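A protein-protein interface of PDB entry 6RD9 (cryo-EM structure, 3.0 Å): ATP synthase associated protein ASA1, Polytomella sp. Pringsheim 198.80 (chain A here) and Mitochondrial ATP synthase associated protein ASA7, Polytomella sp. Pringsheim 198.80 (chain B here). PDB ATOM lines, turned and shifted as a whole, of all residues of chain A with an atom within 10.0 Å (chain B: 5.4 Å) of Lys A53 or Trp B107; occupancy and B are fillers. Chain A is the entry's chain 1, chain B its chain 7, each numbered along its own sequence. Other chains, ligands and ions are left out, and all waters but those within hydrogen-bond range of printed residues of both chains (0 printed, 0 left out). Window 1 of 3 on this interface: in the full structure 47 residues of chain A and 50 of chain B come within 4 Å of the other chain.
The side-chain amino group of Lys A53 lies within salt-bridge range of the side-chain carboxylate of Glu B136 (3.6 Å).
N of Asp B109 lies within hydrogen-bond range of O of Pro A149.
The guanidinium group (NE) of Arg A150 is in hydrogen-bond range of the backbone carbonyl oxygen (O) of Gln B106.
O of Trp B107 sits at hydrogen-bond distance from N of Val A151 (2.9 Å).
The side-chain sulfur (SD) of Met A61 sits close to the backbone carbonyl oxygen (O) of Asp B109 (3.8 Å).
The backbone carbonyl oxygen (O) of Lys A53 is in hydrogen-bond range of the side-chain hydroxyl (OG1) of Thr A57, 2.6 Å away.
The side-chain carboxylate (OE1) of Glu A58 sits close to the side-chain amide oxygen (OE1) of Gln A55 (3.1 Å).
The guanidinium group of Arg A150 lies within salt-bridge range of the side-chain carboxylate of Glu A58, at 2.8 Å.
O of Phe A148 sits at hydrogen-bond distance from NH2 of Arg A150 (3.4 Å).
The backbone carbonyl oxygen (O) of Leu B104 lies within hydrogen-bond range of the side-chain hydroxyl (OH) of Tyr B137 (3.0 Å).
Among the printed residues, pairs that only touch across the chains: Lys A54 with Gln B106 (3.3 Å), Val A153 with Ser B105 (3.3 Å), Arg A150 with Trp B107 (3.3 Å), Val A151 with Pro B108 (3.5 Å), Arg A150 with Pro B108 (3.5 Å), Val A153 with Tyr B137 (3.5 Å), Pro A149 with Pro B108 (3.5 Å), Trp A50 with Trp B107 (3.5 Å), Trp A50 with Leu B103 (3.6 Å), Lys A54 with Trp B107 (3.6 Å), Lys A53 with Trp B107 (3.6 Å), Glu A58 with Pro B108 (3.6 Å), Arg A150 with Asp B109 (3.6 Å), Met A61 with Phe B110 (3.6 Å), Met A61 with Pro B108 (3.7 Å), Trp A50 with Leu B140 (3.7 Å), Thr A57 with Trp B107 (3.8 Å), Val A151 with Tyr B137 (3.8 Å), Arg A150 with Ser B105 (3.8 Å), Val A151 with Asp B109 (3.8 Å), Thr A57 with Ala B133 (3.9 Å), Val A151 with Ser B105 (3.9 Å), Trp A50 with Leu B104 (3.9 Å) and Leu A60 with Ala B133 (3.9 Å).
Printed residues of chain B that touch a printed residue of chain A: Leu B103, Leu B104, Ser B105, Gln B106, Trp B107, Pro B108, Asp B109, Phe B110, Ala B133, Glu B136, Tyr B137 and Leu B140.
Hydrophobic or aromatic side chains of chain B within 4 Å of the printed part of chain A: Leu B103, Leu B104, Trp B107, Pro B108, Ala B133, Tyr B137 and Leu B140.
Along chain B the printed residues that touch a printed residue of chain A span positions 103 to 140.
Of the 24 printed residues of chain A, 11 touch a printed residue of chain B.
Hydrophobic or aromatic side chains of chain A that line the printed part of chain B: Trp A50, Leu A60, Met A61, Val A151 and Val A153.
Among the printed residues, Asp or Glu carboxylates within 4 Å of a Lys or Arg side-chain nitrogen of the other chain: Lys A53 with Glu B136.
Printed residues of chain B within 4 Å of Lys A53: Trp B107 and Glu B136.
Of the printed residues of chain B, Glu A58 touches Pro B108.
Of the printed residues of chain B, Val A151 touches Ser B105, Trp B107, Pro B108, Asp B109 and Tyr B137.
Of the printed residues of chain A, Leu B103 touches Trp A50.
Of chain A, only Trp A50 (3.9 Å) comes within 4 Å of Leu B104.
Trp B107 touches six residues of chain A.
Of the printed residues of chain A, Ala B133 touches Thr A57 (3.9 Å) and Leu A60 (3.9 Å).
Of the printed residues of chain A, Leu B140 touches Trp A50 (3.7 Å).
The nearest residue of chain A that does not touch Trp B107 is Pro A149 (4.4 Å).
The nearest printed residue of chain A that does not touch Asp B109 is Ala A152 (4.8 Å).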
ATOM      1  N   ASN A  45      27.074 -25.456  26.829  1.00  0.00           N
ATOM      2  CA  ASN A  45      27.650 -24.118  26.832  1.00  0.00           C
ATOM      3  C   ASN A  45      27.020 -23.337  25.691  1.00  0.00           C
ATOM      4  O   ASN A  45      27.514 -23.330  24.567  1.00  0.00           O
ATOM      5  CB  ASN A  45      29.161 -24.184  26.704  1.00  0.00           C
ATOM      6  CG  ASN A  45      29.851 -23.213  27.615  1.00  0.00           C
ATOM      7  OD1 ASN A  45      29.388 -22.963  28.720  1.00  0.00           O
ATOM      8  ND2 ASN A  45      30.967 -22.662  27.165  1.00  0.00           N
ATOM      9  N   LEU A  46      25.914 -22.719  25.964  1.00  0.00           N
ATOM     10  CA  LEU A  46      25.320 -21.835  24.981  1.00  0.00           C
ATOM     11  C   LEU A  46      24.893 -20.519  25.586  1.00  0.00           C
ATOM     12  O   LEU A  46      24.925 -19.505  24.906  1.00  0.00           O
ATOM     13  CB  LEU A  46      24.151 -22.516  24.297  1.00  0.00           C
ATOM     14  CG  LEU A  46      23.443 -21.805  23.162  1.00  0.00           C
ATOM     15  CD1 LEU A  46      23.282 -22.742  22.028  1.00  0.00           C
ATOM     16  CD2 LEU A  46      22.100 -21.366  23.630  1.00  0.00           C
ATOM     17  N   VAL A  47      24.502 -20.499  26.851  1.00  0.00           N
ATOM     18  CA  VAL A  47      24.367 -19.217  27.525  1.00  0.00           C
ATOM     19  C   VAL A  47      25.738 -18.583  27.708  1.00  0.00           C
ATOM     20  O   VAL A  47      25.893 -17.366  27.588  1.00  0.00           O
ATOM     21  CB  VAL A  47      23.603 -19.398  28.849  1.00  0.00           C
ATOM     22  CG1 VAL A  47      23.663 -18.169  29.723  1.00  0.00           C
ATOM     23  CG2 VAL A  47      22.168 -19.719  28.553  1.00  0.00           C
ATOM     24  N   ASN A  48      26.771 -19.397  27.916  1.00  0.00           N
ATOM     25  CA  ASN A  48      28.121 -18.854  28.003  1.00  0.00           C
ATOM     26  C   ASN A  48      28.798 -18.686  26.658  1.00  0.00           C
ATOM     27  O   ASN A  48      29.820 -18.010  26.604  1.00  0.00           O
ATOM     28  CB  ASN A  48      29.009 -19.724  28.882  1.00  0.00           C
ATOM     29  CG  ASN A  48      28.726 -19.541  30.342  1.00  0.00           C
ATOM     30  OD1 ASN A  48      28.477 -20.503  31.060  1.00  0.00           O
ATOM     31  ND2 ASN A  48      28.755 -18.298  30.797  1.00  0.00           N
ATOM     32  N   GLU A  49      28.295 -19.283  25.585  1.00  0.00           N
ATOM     33  CA  GLU A  49      28.800 -18.920  24.269  1.00  0.00           C
ATOM     34  C   GLU A  49      28.071 -17.744  23.667  1.00  0.00           C
ATOM     35  O   GLU A  49      28.676 -16.971  22.930  1.00  0.00           O
ATOM     36  CB  GLU A  49      28.713 -20.082  23.297  1.00  0.00           C
ATOM     37  CG  GLU A  49      29.758 -21.112  23.535  1.00  0.00           C
ATOM     38  CD  GLU A  49      29.691 -22.235  22.534  1.00  0.00           C
ATOM     39  OE1 GLU A  49      28.741 -22.254  21.727  1.00  0.00           O
ATOM     40  OE2 GLU A  49      30.590 -23.099  22.554  1.00  0.00           O
ATOM     41  N   TRP A  50      26.790 -17.584  23.948  1.00  0.00           N
ATOM     42  CA  TRP A  50      26.089 -16.434  23.418  1.00  0.00           C
ATOM     43  C   TRP A  50      26.326 -15.202  24.254  1.00  0.00           C
ATOM     44  O   TRP A  50      26.003 -14.104  23.810  1.00  0.00           O
ATOM     45  CB  TRP A  50      24.596 -16.696  23.326  1.00  0.00           C
ATOM     46  CG  TRP A  50      24.204 -17.633  22.264  1.00  0.00           C
ATOM     47  CD1 TRP A  50      25.010 -18.440  21.547  1.00  0.00           C
ATOM     48  CD2 TRP A  50      22.886 -17.860  21.792  1.00  0.00           C
ATOM     49  NE1 TRP A  50      24.283 -19.165  20.656  1.00  0.00           N
ATOM     50  CE2 TRP A  50      22.967 -18.825  20.789  1.00  0.00           C
ATOM     51  CE3 TRP A  50      21.643 -17.342  22.122  1.00  0.00           C
ATOM     52  CZ2 TRP A  50      21.857 -19.273  20.111  1.00  0.00           C
ATOM     53  CZ3 TRP A  50      20.555 -17.786  21.459  1.00  0.00           C
ATOM     54  CH2 TRP A  50      20.661 -18.733  20.457  1.00  0.00           C
ATOM     55  N   ASN A  51      26.840 -15.350  25.462  1.00  0.00           N
ATOM     56  CA  ASN A  51      27.287 -14.176  26.188  1.00  0.00           C
ATOM     57  C   ASN A  51      28.672 -13.749  25.760  1.00  0.00           C
ATOM     58  O   ASN A  51      29.030 -12.588  25.945  1.00  0.00           O
ATOM     59  CB  ASN A  51      27.267 -14.427  27.688  1.00  0.00           C
ATOM     60  CG  ASN A  51      25.910 -14.221  28.278  1.00  0.00           C
ATOM     61  OD1 ASN A  51      25.130 -13.419  27.784  1.00  0.00           O
ATOM     62  ND2 ASN A  51      25.612 -14.943  29.337  1.00  0.00           N
ATOM     63  N   ASN A  52      29.455 -14.667  25.205  1.00  0.00           N
ATOM     64  CA  ASN A  52      30.725 -14.289  24.610  1.00  0.00           C
ATOM     65  C   ASN A  52      30.512 -13.547  23.310  1.00  0.00           C
ATOM     66  O   ASN A  52      31.247 -12.609  23.002  1.00  0.00           O
ATOM     67  CB  ASN A  52      31.574 -15.522  24.371  1.00  0.00           C
ATOM     68  CG  ASN A  52      32.074 -16.118  25.635  1.00  0.00           C
ATOM     69  OD1 ASN A  52      32.058 -15.482  26.681  1.00  0.00           O
ATOM     70  ND2 ASN A  52      32.532 -17.352  25.557  1.00  0.00           N
ATOM     71  N   LYS A  53      29.522 -13.959  22.531  1.00  0.00           N
ATOM     72  CA  LYS A  53      29.241 -13.285  21.280  1.00  0.00           C
ATOM     73  C   LYS A  53      28.643 -11.916  21.506  1.00  0.00           C
ATOM     74  O   LYS A  53      28.878 -11.011  20.708  1.00  0.00           O
ATOM     75  CB  LYS A  53      28.311 -14.132  20.439  1.00  0.00           C
ATOM     76  CG  LYS A  53      28.912 -15.424  20.040  1.00  0.00           C
ATOM     77  CD  LYS A  53      27.900 -16.301  19.396  1.00  0.00           C
ATOM     78  CE  LYS A  53      28.559 -17.529  18.872  1.00  0.00           C
ATOM     79  NZ  LYS A  53      27.663 -18.240  17.955  1.00  0.00           N
ATOM     80  N   LYS A  54      27.866 -11.741  22.565  1.00  0.00           N
ATOM     81  CA  LYS A  54      27.386 -10.411  22.899  1.00  0.00           C
ATOM     82  C   LYS A  54      28.521  -9.543  23.394  1.00  0.00           C
ATOM     83  O   LYS A  54      28.513  -8.331  23.177  1.00  0.00           O
ATOM     84  CB  LYS A  54      26.277 -10.507  23.942  1.00  0.00           C
ATOM     85  CG  LYS A  54      25.660  -9.214  24.363  1.00  0.00           C
ATOM     86  CD  LYS A  54      24.925  -9.379  25.650  1.00  0.00           C
ATOM     87  CE  LYS A  54      25.127  -8.176  26.525  1.00  0.00           C
ATOM     88  NZ  LYS A  54      24.336  -8.254  27.776  1.00  0.00           N
ATOM     89  N   GLN A  55      29.515 -10.142  24.037  1.00  0.00           N
ATOM     90  CA  GLN A  55      30.660  -9.370  24.487  1.00  0.00           C
ATOM     91  C   GLN A  55      31.639  -9.115  23.362  1.00  0.00           C
ATOM     92  O   GLN A  55      32.294  -8.077  23.356  1.00  0.00           O
ATOM     93  CB  GLN A  55      31.354 -10.075  25.641  1.00  0.00           C
ATOM     94  CG  GLN A  55      32.149  -9.143  26.506  1.00  0.00           C
ATOM     95  CD  GLN A  55      31.332  -7.964  26.989  1.00  0.00           C
ATOM     96  OE1 GLN A  55      30.210  -8.119  27.473  1.00  0.00           O
ATOM     97  NE2 GLN A  55      31.894  -6.772  26.861  1.00  0.00           N
ATOM     98  N   ALA A  56      31.752 -10.036  22.411  1.00  0.00           N
ATOM     99  CA  ALA A  56      32.565  -9.787  21.231  1.00  0.00           C
ATOM    100  C   ALA A  56      31.972  -8.681  20.381  1.00  0.00           C
ATOM    101  O   ALA A  56      32.701  -7.856  19.836  1.00  0.00           O
ATOM    102  CB  ALA A  56      32.702 -11.062  20.414  1.00  0.00           C
ATOM    103  N   THR A  57      30.653  -8.640  20.267  1.00  0.00           N
ATOM    104  CA  THR A  57      30.000  -7.575  19.524  1.00  0.00           C
ATOM    105  C   THR A  57      30.046  -6.257  20.277  1.00  0.00           C
ATOM    106  O   THR A  57      30.077  -5.200  19.657  1.00  0.00           O
ATOM    107  CB  THR A  57      28.568  -7.984  19.217  1.00  0.00           C
ATOM    108  OG1 THR A  57      28.574  -9.333  18.758  1.00  0.00           O
ATOM    109  CG2 THR A  57      27.974  -7.133  18.148  1.00  0.00           C
ATOM    110  N   GLU A  58      30.044  -6.281  21.604  1.00  0.00           N
ATOM    111  CA  GLU A  58      30.244  -5.035  22.330  1.00  0.00           C
ATOM    112  C   GLU A  58      31.695  -4.606  22.295  1.00  0.00           C
ATOM    113  O   GLU A  58      31.987  -3.420  22.427  1.00  0.00           O
ATOM    114  CB  GLU A  58      29.767  -5.170  23.768  1.00  0.00           C
ATOM    115  CG  GLU A  58      28.278  -5.030  23.919  1.00  0.00           C
ATOM    116  CD  GLU A  58      27.782  -5.343  25.308  1.00  0.00           C
ATOM    117  OE1 GLU A  58      28.576  -5.846  26.125  1.00  0.00           O
ATOM    118  OE2 GLU A  58      26.592  -5.094  25.582  1.00  0.00           O
ATOM    119  N   ASN A  59      32.617  -5.545  22.135  1.00  0.00           N
ATOM    120  CA  ASN A  59      34.010  -5.170  21.969  1.00  0.00           C
ATOM    121  C   ASN A  59      34.259  -4.593  20.592  1.00  0.00           C
ATOM    122  O   ASN A  59      35.034  -3.648  20.445  1.00  0.00           O
ATOM    123  CB  ASN A  59      34.910  -6.369  22.179  1.00  0.00           C
ATOM    124  CG  ASN A  59      35.051  -6.731  23.610  1.00  0.00           C
ATOM    125  OD1 ASN A  59      34.618  -5.997  24.491  1.00  0.00           O
ATOM    126  ND2 ASN A  59      35.660  -7.875  23.864  1.00  0.00           N
ATOM    127  N   LEU A  60      33.629  -5.159  19.571  1.00  0.00           N
ATOM    128  CA  LEU A  60      33.793  -4.639  18.224  1.00  0.00           C
ATOM    129  C   LEU A  60      33.134  -3.289  18.076  1.00  0.00           C
ATOM    130  O   LEU A  60      33.677  -2.409  17.420  1.00  0.00           O
ATOM    131  CB  LEU A  60      33.214  -5.604  17.210  1.00  0.00           C
ATOM    132  CG  LEU A  60      34.088  -6.798  16.914  1.00  0.00           C
ATOM    133  CD1 LEU A  60      33.245  -7.883  16.314  1.00  0.00           C
ATOM    134  CD2 LEU A  60      35.177  -6.385  15.974  1.00  0.00           C
ATOM    135  N   MET A  61      31.970  -3.103  18.675  1.00  0.00           N
ATOM    136  CA  MET A  61      31.308  -1.815  18.592  1.00  0.00           C
ATOM    137  C   MET A  61      32.040  -0.761  19.400  1.00  0.00           C
ATOM    138  O   MET A  61      31.976   0.420  19.068  1.00  0.00           O
ATOM    139  CB  MET A  61      29.866  -1.940  19.063  1.00  0.00           C
ATOM    140  CG  MET A  61      28.954  -2.591  18.071  1.00  0.00           C
ATOM    141  SD  MET A  61      27.254  -2.574  18.581  1.00  0.00           S
ATOM    142  CE  MET A  61      27.031  -0.854  18.936  1.00  0.00           C
ATOM    143  N   ALA A 147      27.812   2.111  26.470  1.00  0.00           N
ATOM    144  CA  ALA A 147      26.395   2.410  26.666  1.00  0.00           C
ATOM    145  C   ALA A 147      25.751   2.460  25.291  1.00  0.00           C
ATOM    146  O   ALA A 147      25.486   3.532  24.751  1.00  0.00           O
ATOM    147  CB  ALA A 147      26.210   3.695  27.409  1.00  0.00           C
ATOM    148  N   PHE A 148      25.472   1.300  24.742  1.00  0.00           N
ATOM    149  CA  PHE A 148      24.899   1.233  23.419  1.00  0.00           C
ATOM    150  C   PHE A 148      23.416   0.935  23.520  1.00  0.00           C
ATOM    151  O   PHE A 148      22.980   0.293  24.475  1.00  0.00           O
ATOM    152  CB  PHE A 148      25.569   0.138  22.582  1.00  0.00           C
ATOM    153  CG  PHE A 148      27.015   0.376  22.320  1.00  0.00           C
ATOM    154  CD1 PHE A 148      27.451   1.587  21.839  1.00  0.00           C
ATOM    155  CD2 PHE A 148      27.939  -0.615  22.557  1.00  0.00           C
ATOM    156  CE1 PHE A 148      28.777   1.805  21.599  1.00  0.00           C
ATOM    157  CE2 PHE A 148      29.267  -0.399  22.321  1.00  0.00           C
ATOM    158  CZ  PHE A 148      29.684   0.812  21.841  1.00  0.00           C
ATOM    159  N   PRO A 149      22.608   1.387  22.572  1.00  0.00           N
ATOM    160  CA  PRO A 149      21.217   0.946  22.543  1.00  0.00           C
ATOM    161  C   PRO A 149      21.135  -0.508  22.130  1.00  0.00           C
ATOM    162  O   PRO A 149      22.029  -1.053  21.488  1.00  0.00           O
ATOM    163  CB  PRO A 149      20.576   1.860  21.501  1.00  0.00           C
ATOM    164  CG  PRO A 149      21.681   2.275  20.654  1.00  0.00           C
ATOM    165  CD  PRO A 149      22.879   2.379  21.526  1.00  0.00           C
ATOM    166  N   ARG A 150      20.045  -1.142  22.520  1.00  0.00           N
ATOM    167  CA  ARG A 150      19.847  -2.555  22.264  1.00  0.00           C
ATOM    168  C   ARG A 150      19.032  -2.758  21.002  1.00  0.00           C
ATOM    169  O   ARG A 150      18.340  -1.854  20.538  1.00  0.00           O
ATOM    170  CB  ARG A 150      19.160  -3.211  23.457  1.00  0.00           C
ATOM    171  CG  ARG A 150      20.011  -3.237  24.694  1.00  0.00           C
ATOM    172  CD  ARG A 150      21.310  -3.874  24.334  1.00  0.00           C
ATOM    173  NE  ARG A 150      22.204  -4.142  25.438  1.00  0.00           N
ATOM    174  CZ  ARG A 150      23.444  -3.691  25.497  1.00  0.00           C
ATOM    175  NH1 ARG A 150      24.212  -3.989  26.528  1.00  0.00           N
ATOM    176  NH2 ARG A 150      23.906  -2.929  24.531  1.00  0.00           N
ATOM    177  N   VAL A 151      19.140  -3.955  20.433  1.00  0.00           N
ATOM    178  CA  VAL A 151      18.374  -4.273  19.241  1.00  0.00           C
ATOM    179  C   VAL A 151      16.907  -4.360  19.615  1.00  0.00           C
ATOM    180  O   VAL A 151      16.544  -5.022  20.591  1.00  0.00           O
ATOM    181  CB  VAL A 151      18.857  -5.585  18.617  1.00  0.00           C
ATOM    182  CG1 VAL A 151      18.137  -5.824  17.350  1.00  0.00           C
ATOM    183  CG2 VAL A 151      20.293  -5.509  18.326  1.00  0.00           C
ATOM    184  N   ALA A 152      16.064  -3.659  18.875  1.00  0.00           N
ATOM    185  CA  ALA A 152      14.635  -3.710  19.125  1.00  0.00           C
ATOM    186  C   ALA A 152      14.106  -5.063  18.704  1.00  0.00           C
ATOM    187  O   ALA A 152      14.060  -5.381  17.517  1.00  0.00           O
ATOM    188  CB  ALA A 152      13.920  -2.603  18.367  1.00  0.00           C
ATOM    189  N   VAL A 153      13.724  -5.867  19.680  1.00  0.00           N
ATOM    190  CA  VAL A 153      13.033  -7.128  19.450  1.00  0.00           C
ATOM    191  C   VAL A 153      11.687  -7.009  20.140  1.00  0.00           C
ATOM    192  O   VAL A 153      11.531  -6.194  21.063  1.00  0.00           O
ATOM    193  CB  VAL A 153      13.854  -8.326  19.970  1.00  0.00           C
ATOM    194  CG1 VAL A 153      15.091  -8.460  19.180  1.00  0.00           C
ATOM    195  CG2 VAL A 153      14.213  -8.083  21.356  1.00  0.00           C
ATOM    196  N   LEU B 103      18.237 -13.093  26.039  1.00  0.00           N
ATOM    197  CA  LEU B 103      19.604 -12.626  25.941  1.00  0.00           C
ATOM    198  C   LEU B 103      19.997 -12.226  24.532  1.00  0.00           C
ATOM    199  O   LEU B 103      21.063 -11.639  24.352  1.00  0.00           O
ATOM    200  CB  LEU B 103      20.565 -13.669  26.506  1.00  0.00           C
ATOM    201  CG  LEU B 103      20.635 -15.120  26.082  1.00  0.00           C
ATOM    202  CD1 LEU B 103      21.613 -15.272  25.006  1.00  0.00           C
ATOM    203  CD2 LEU B 103      21.106 -15.908  27.254  1.00  0.00           C
ATOM    204  N   LEU B 104      19.181 -12.535  23.536  1.00  0.00           N
ATOM    205  CA  LEU B 104      19.247 -11.837  22.269  1.00  0.00           C
ATOM    206  C   LEU B 104      18.481 -10.532  22.300  1.00  0.00           C
ATOM    207  O   LEU B 104      18.578  -9.756  21.354  1.00  0.00           O
ATOM    208  CB  LEU B 104      18.693 -12.706  21.158  1.00  0.00           C
ATOM    209  CG  LEU B 104      19.386 -14.025  20.925  1.00  0.00           C
ATOM    210  CD1 LEU B 104      18.786 -14.654  19.760  1.00  0.00           C
ATOM    211  CD2 LEU B 104      20.803 -13.797  20.650  1.00  0.00           C
ATOM    212  N   SER B 105      17.703 -10.281  23.339  1.00  0.00           N
ATOM    213  CA  SER B 105      17.100  -8.977  23.523  1.00  0.00           C
ATOM    214  C   SER B 105      18.089  -7.949  24.006  1.00  0.00           C
ATOM    215  O   SER B 105      17.834  -6.754  23.868  1.00  0.00           O
ATOM    216  CB  SER B 105      15.971  -9.051  24.537  1.00  0.00           C
ATOM    217  OG  SER B 105      14.915  -9.817  24.036  1.00  0.00           O
ATOM    218  N   GLN B 106      19.193  -8.390  24.590  1.00  0.00           N
ATOM    219  CA  GLN B 106      20.152  -7.517  25.233  1.00  0.00           C
ATOM    220  C   GLN B 106      21.415  -7.374  24.421  1.00  0.00           C
ATOM    221  O   GLN B 106      22.472  -7.083  24.978  1.00  0.00           O
ATOM    222  CB  GLN B 106      20.472  -8.038  26.626  1.00  0.00           C
ATOM    223  CG  GLN B 106      19.297  -7.964  27.562  1.00  0.00           C
ATOM    224  CD  GLN B 106      18.774  -6.558  27.698  1.00  0.00           C
ATOM    225  OE1 GLN B 106      17.589  -6.302  27.507  1.00  0.00           O
ATOM    226  NE2 GLN B 106      19.660  -5.631  28.032  1.00  0.00           N
ATOM    227  N   TRP B 107      21.328  -7.567  23.133  1.00  0.00           N
ATOM    228  CA  TRP B 107      22.353  -7.461  22.122  1.00  0.00           C
ATOM    229  C   TRP B 107      22.463  -6.017  21.674  1.00  0.00           C
ATOM    230  O   TRP B 107      21.442  -5.376  21.432  1.00  0.00           O
ATOM    231  CB  TRP B 107      21.995  -8.326  20.941  1.00  0.00           C
ATOM    232  CG  TRP B 107      23.121  -8.953  20.277  1.00  0.00           C
ATOM    233  CD1 TRP B 107      23.855  -8.438  19.285  1.00  0.00           C
ATOM    234  CD2 TRP B 107      23.634 -10.252  20.529  1.00  0.00           C
ATOM    235  NE1 TRP B 107      24.816  -9.320  18.902  1.00  0.00           N
ATOM    236  CE2 TRP B 107      24.693 -10.452  19.650  1.00  0.00           C
ATOM    237  CE3 TRP B 107      23.301 -11.264  21.419  1.00  0.00           C
ATOM    238  CZ2 TRP B 107      25.426 -11.609  19.635  1.00  0.00           C
ATOM    239  CZ3 TRP B 107      24.024 -12.415  21.397  1.00  0.00           C
ATOM    240  CH2 TRP B 107      25.069 -12.583  20.510  1.00  0.00           C
ATOM    241  N   PRO B 108      23.678  -5.489  21.561  1.00  0.00           N
ATOM    242  CA  PRO B 108      23.847  -4.082  21.211  1.00  0.00           C
ATOM    243  C   PRO B 108      23.453  -3.818  19.776  1.00  0.00           C
ATOM    244  O   PRO B 108      23.650  -4.652  18.895  1.00  0.00           O
ATOM    245  CB  PRO B 108      25.338  -3.861  21.418  1.00  0.00           C
ATOM    246  CG  PRO B 108      25.909  -5.170  21.184  1.00  0.00           C
ATOM    247  CD  PRO B 108      24.972  -6.150  21.741  1.00  0.00           C
ATOM    248  N   ASP B 109      22.872  -2.648  19.541  1.00  0.00           N
ATOM    249  CA  ASP B 109      22.396  -2.321  18.202  1.00  0.00           C
ATOM    250  C   ASP B 109      23.588  -2.057  17.309  1.00  0.00           C
ATOM    251  O   ASP B 109      24.131  -0.955  17.276  1.00  0.00           O
ATOM    252  CB  ASP B 109      21.472  -1.119  18.215  1.00  0.00           C
ATOM    253  CG  ASP B 109      20.472  -1.161  17.100  1.00  0.00           C
ATOM    254  OD1 ASP B 109      19.367  -0.627  17.273  1.00  0.00           O
ATOM    255  OD2 ASP B 109      20.774  -1.750  16.053  1.00  0.00           O
ATOM    256  N   PHE B 110      23.993  -3.075  16.572  1.00  0.00           N
ATOM    257  CA  PHE B 110      25.105  -2.930  15.661  1.00  0.00           C
ATOM    258  C   PHE B 110      24.755  -2.106  14.446  1.00  0.00           C
ATOM    259  O   PHE B 110      25.655  -1.600  13.791  1.00  0.00           O
ATOM    260  CB  PHE B 110      25.608  -4.301  15.225  1.00  0.00           C
ATOM    261  CG  PHE B 110      24.529  -5.291  14.996  1.00  0.00           C
ATOM    262  CD1 PHE B 110      24.222  -6.218  15.950  1.00  0.00           C
ATOM    263  CD2 PHE B 110      23.827  -5.296  13.825  1.00  0.00           C
ATOM    264  CE1 PHE B 110      23.231  -7.111  15.743  1.00  0.00           C
ATOM    265  CE2 PHE B 110      22.838  -6.197  13.618  1.00  0.00           C
ATOM    266  CZ  PHE B 110      22.542  -7.097  14.575  1.00  0.00           C
ATOM    267  N   ALA B 133      29.891 -10.298  12.792  1.00  0.00           N
ATOM    268  CA  ALA B 133      29.180 -10.392  14.054  1.00  0.00           C
ATOM    269  C   ALA B 133      27.756  -9.896  13.924  1.00  0.00           C
ATOM    270  O   ALA B 133      26.929 -10.155  14.795  1.00  0.00           O
ATOM    271  CB  ALA B 133      29.916  -9.606  15.126  1.00  0.00           C
ATOM    272  N   GLU B 136      25.959 -12.895  12.276  1.00  0.00           N
ATOM    273  CA  GLU B 136      25.848 -13.971  13.240  1.00  0.00           C
ATOM    274  C   GLU B 136      24.624 -13.800  14.105  1.00  0.00           C
ATOM    275  O   GLU B 136      23.969 -14.783  14.439  1.00  0.00           O
ATOM    276  CB  GLU B 136      27.094 -13.990  14.096  1.00  0.00           C
ATOM    277  CG  GLU B 136      27.094 -14.921  15.234  1.00  0.00           C
ATOM    278  CD  GLU B 136      28.093 -14.475  16.250  1.00  0.00           C
ATOM    279  OE1 GLU B 136      27.924 -13.358  16.777  1.00  0.00           O
ATOM    280  OE2 GLU B 136      29.065 -15.206  16.494  1.00  0.00           O
ATOM    281  N   TYR B 137      24.295 -12.561  14.459  1.00  0.00           N
ATOM    282  CA  TYR B 137      23.094 -12.295  15.233  1.00  0.00           C
ATOM    283  C   TYR B 137      21.854 -12.677  14.462  1.00  0.00           C
ATOM    284  O   TYR B 137      20.889 -13.160  15.043  1.00  0.00           O
ATOM    285  CB  TYR B 137      23.013 -10.831  15.601  1.00  0.00           C
ATOM    286  CG  TYR B 137      21.758 -10.462  16.330  1.00  0.00           C
ATOM    287  CD1 TYR B 137      21.635 -10.719  17.671  1.00  0.00           C
ATOM    288  CD2 TYR B 137      20.706  -9.842  15.687  1.00  0.00           C
ATOM    289  CE1 TYR B 137      20.513 -10.381  18.341  1.00  0.00           C
ATOM    290  CE2 TYR B 137      19.587  -9.516  16.353  1.00  0.00           C
ATOM    291  CZ  TYR B 137      19.502  -9.784  17.680  1.00  0.00           C
ATOM    292  OH  TYR B 137      18.389  -9.457  18.381  1.00  0.00           O
ATOM    293  N   LEU B 140      21.545 -16.367  14.867  1.00  0.00           N
ATOM    294  CA  LEU B 140      21.059 -16.785  16.170  1.00  0.00           C
ATOM    295  C   LEU B 140      19.610 -16.398  16.361  1.00  0.00           C
ATOM    296  O   LEU B 140      18.844 -17.147  16.955  1.00  0.00           O
ATOM    297  CB  LEU B 140      21.892 -16.155  17.275  1.00  0.00           C
ATOM    298  CG  LEU B 140      23.390 -16.332  17.254  1.00  0.00           C
ATOM    299  CD1 LEU B 140      23.995 -15.591  18.399  1.00  0.00           C
ATOM    300  CD2 LEU B 140      23.712 -17.773  17.307  1.00  0.00           C
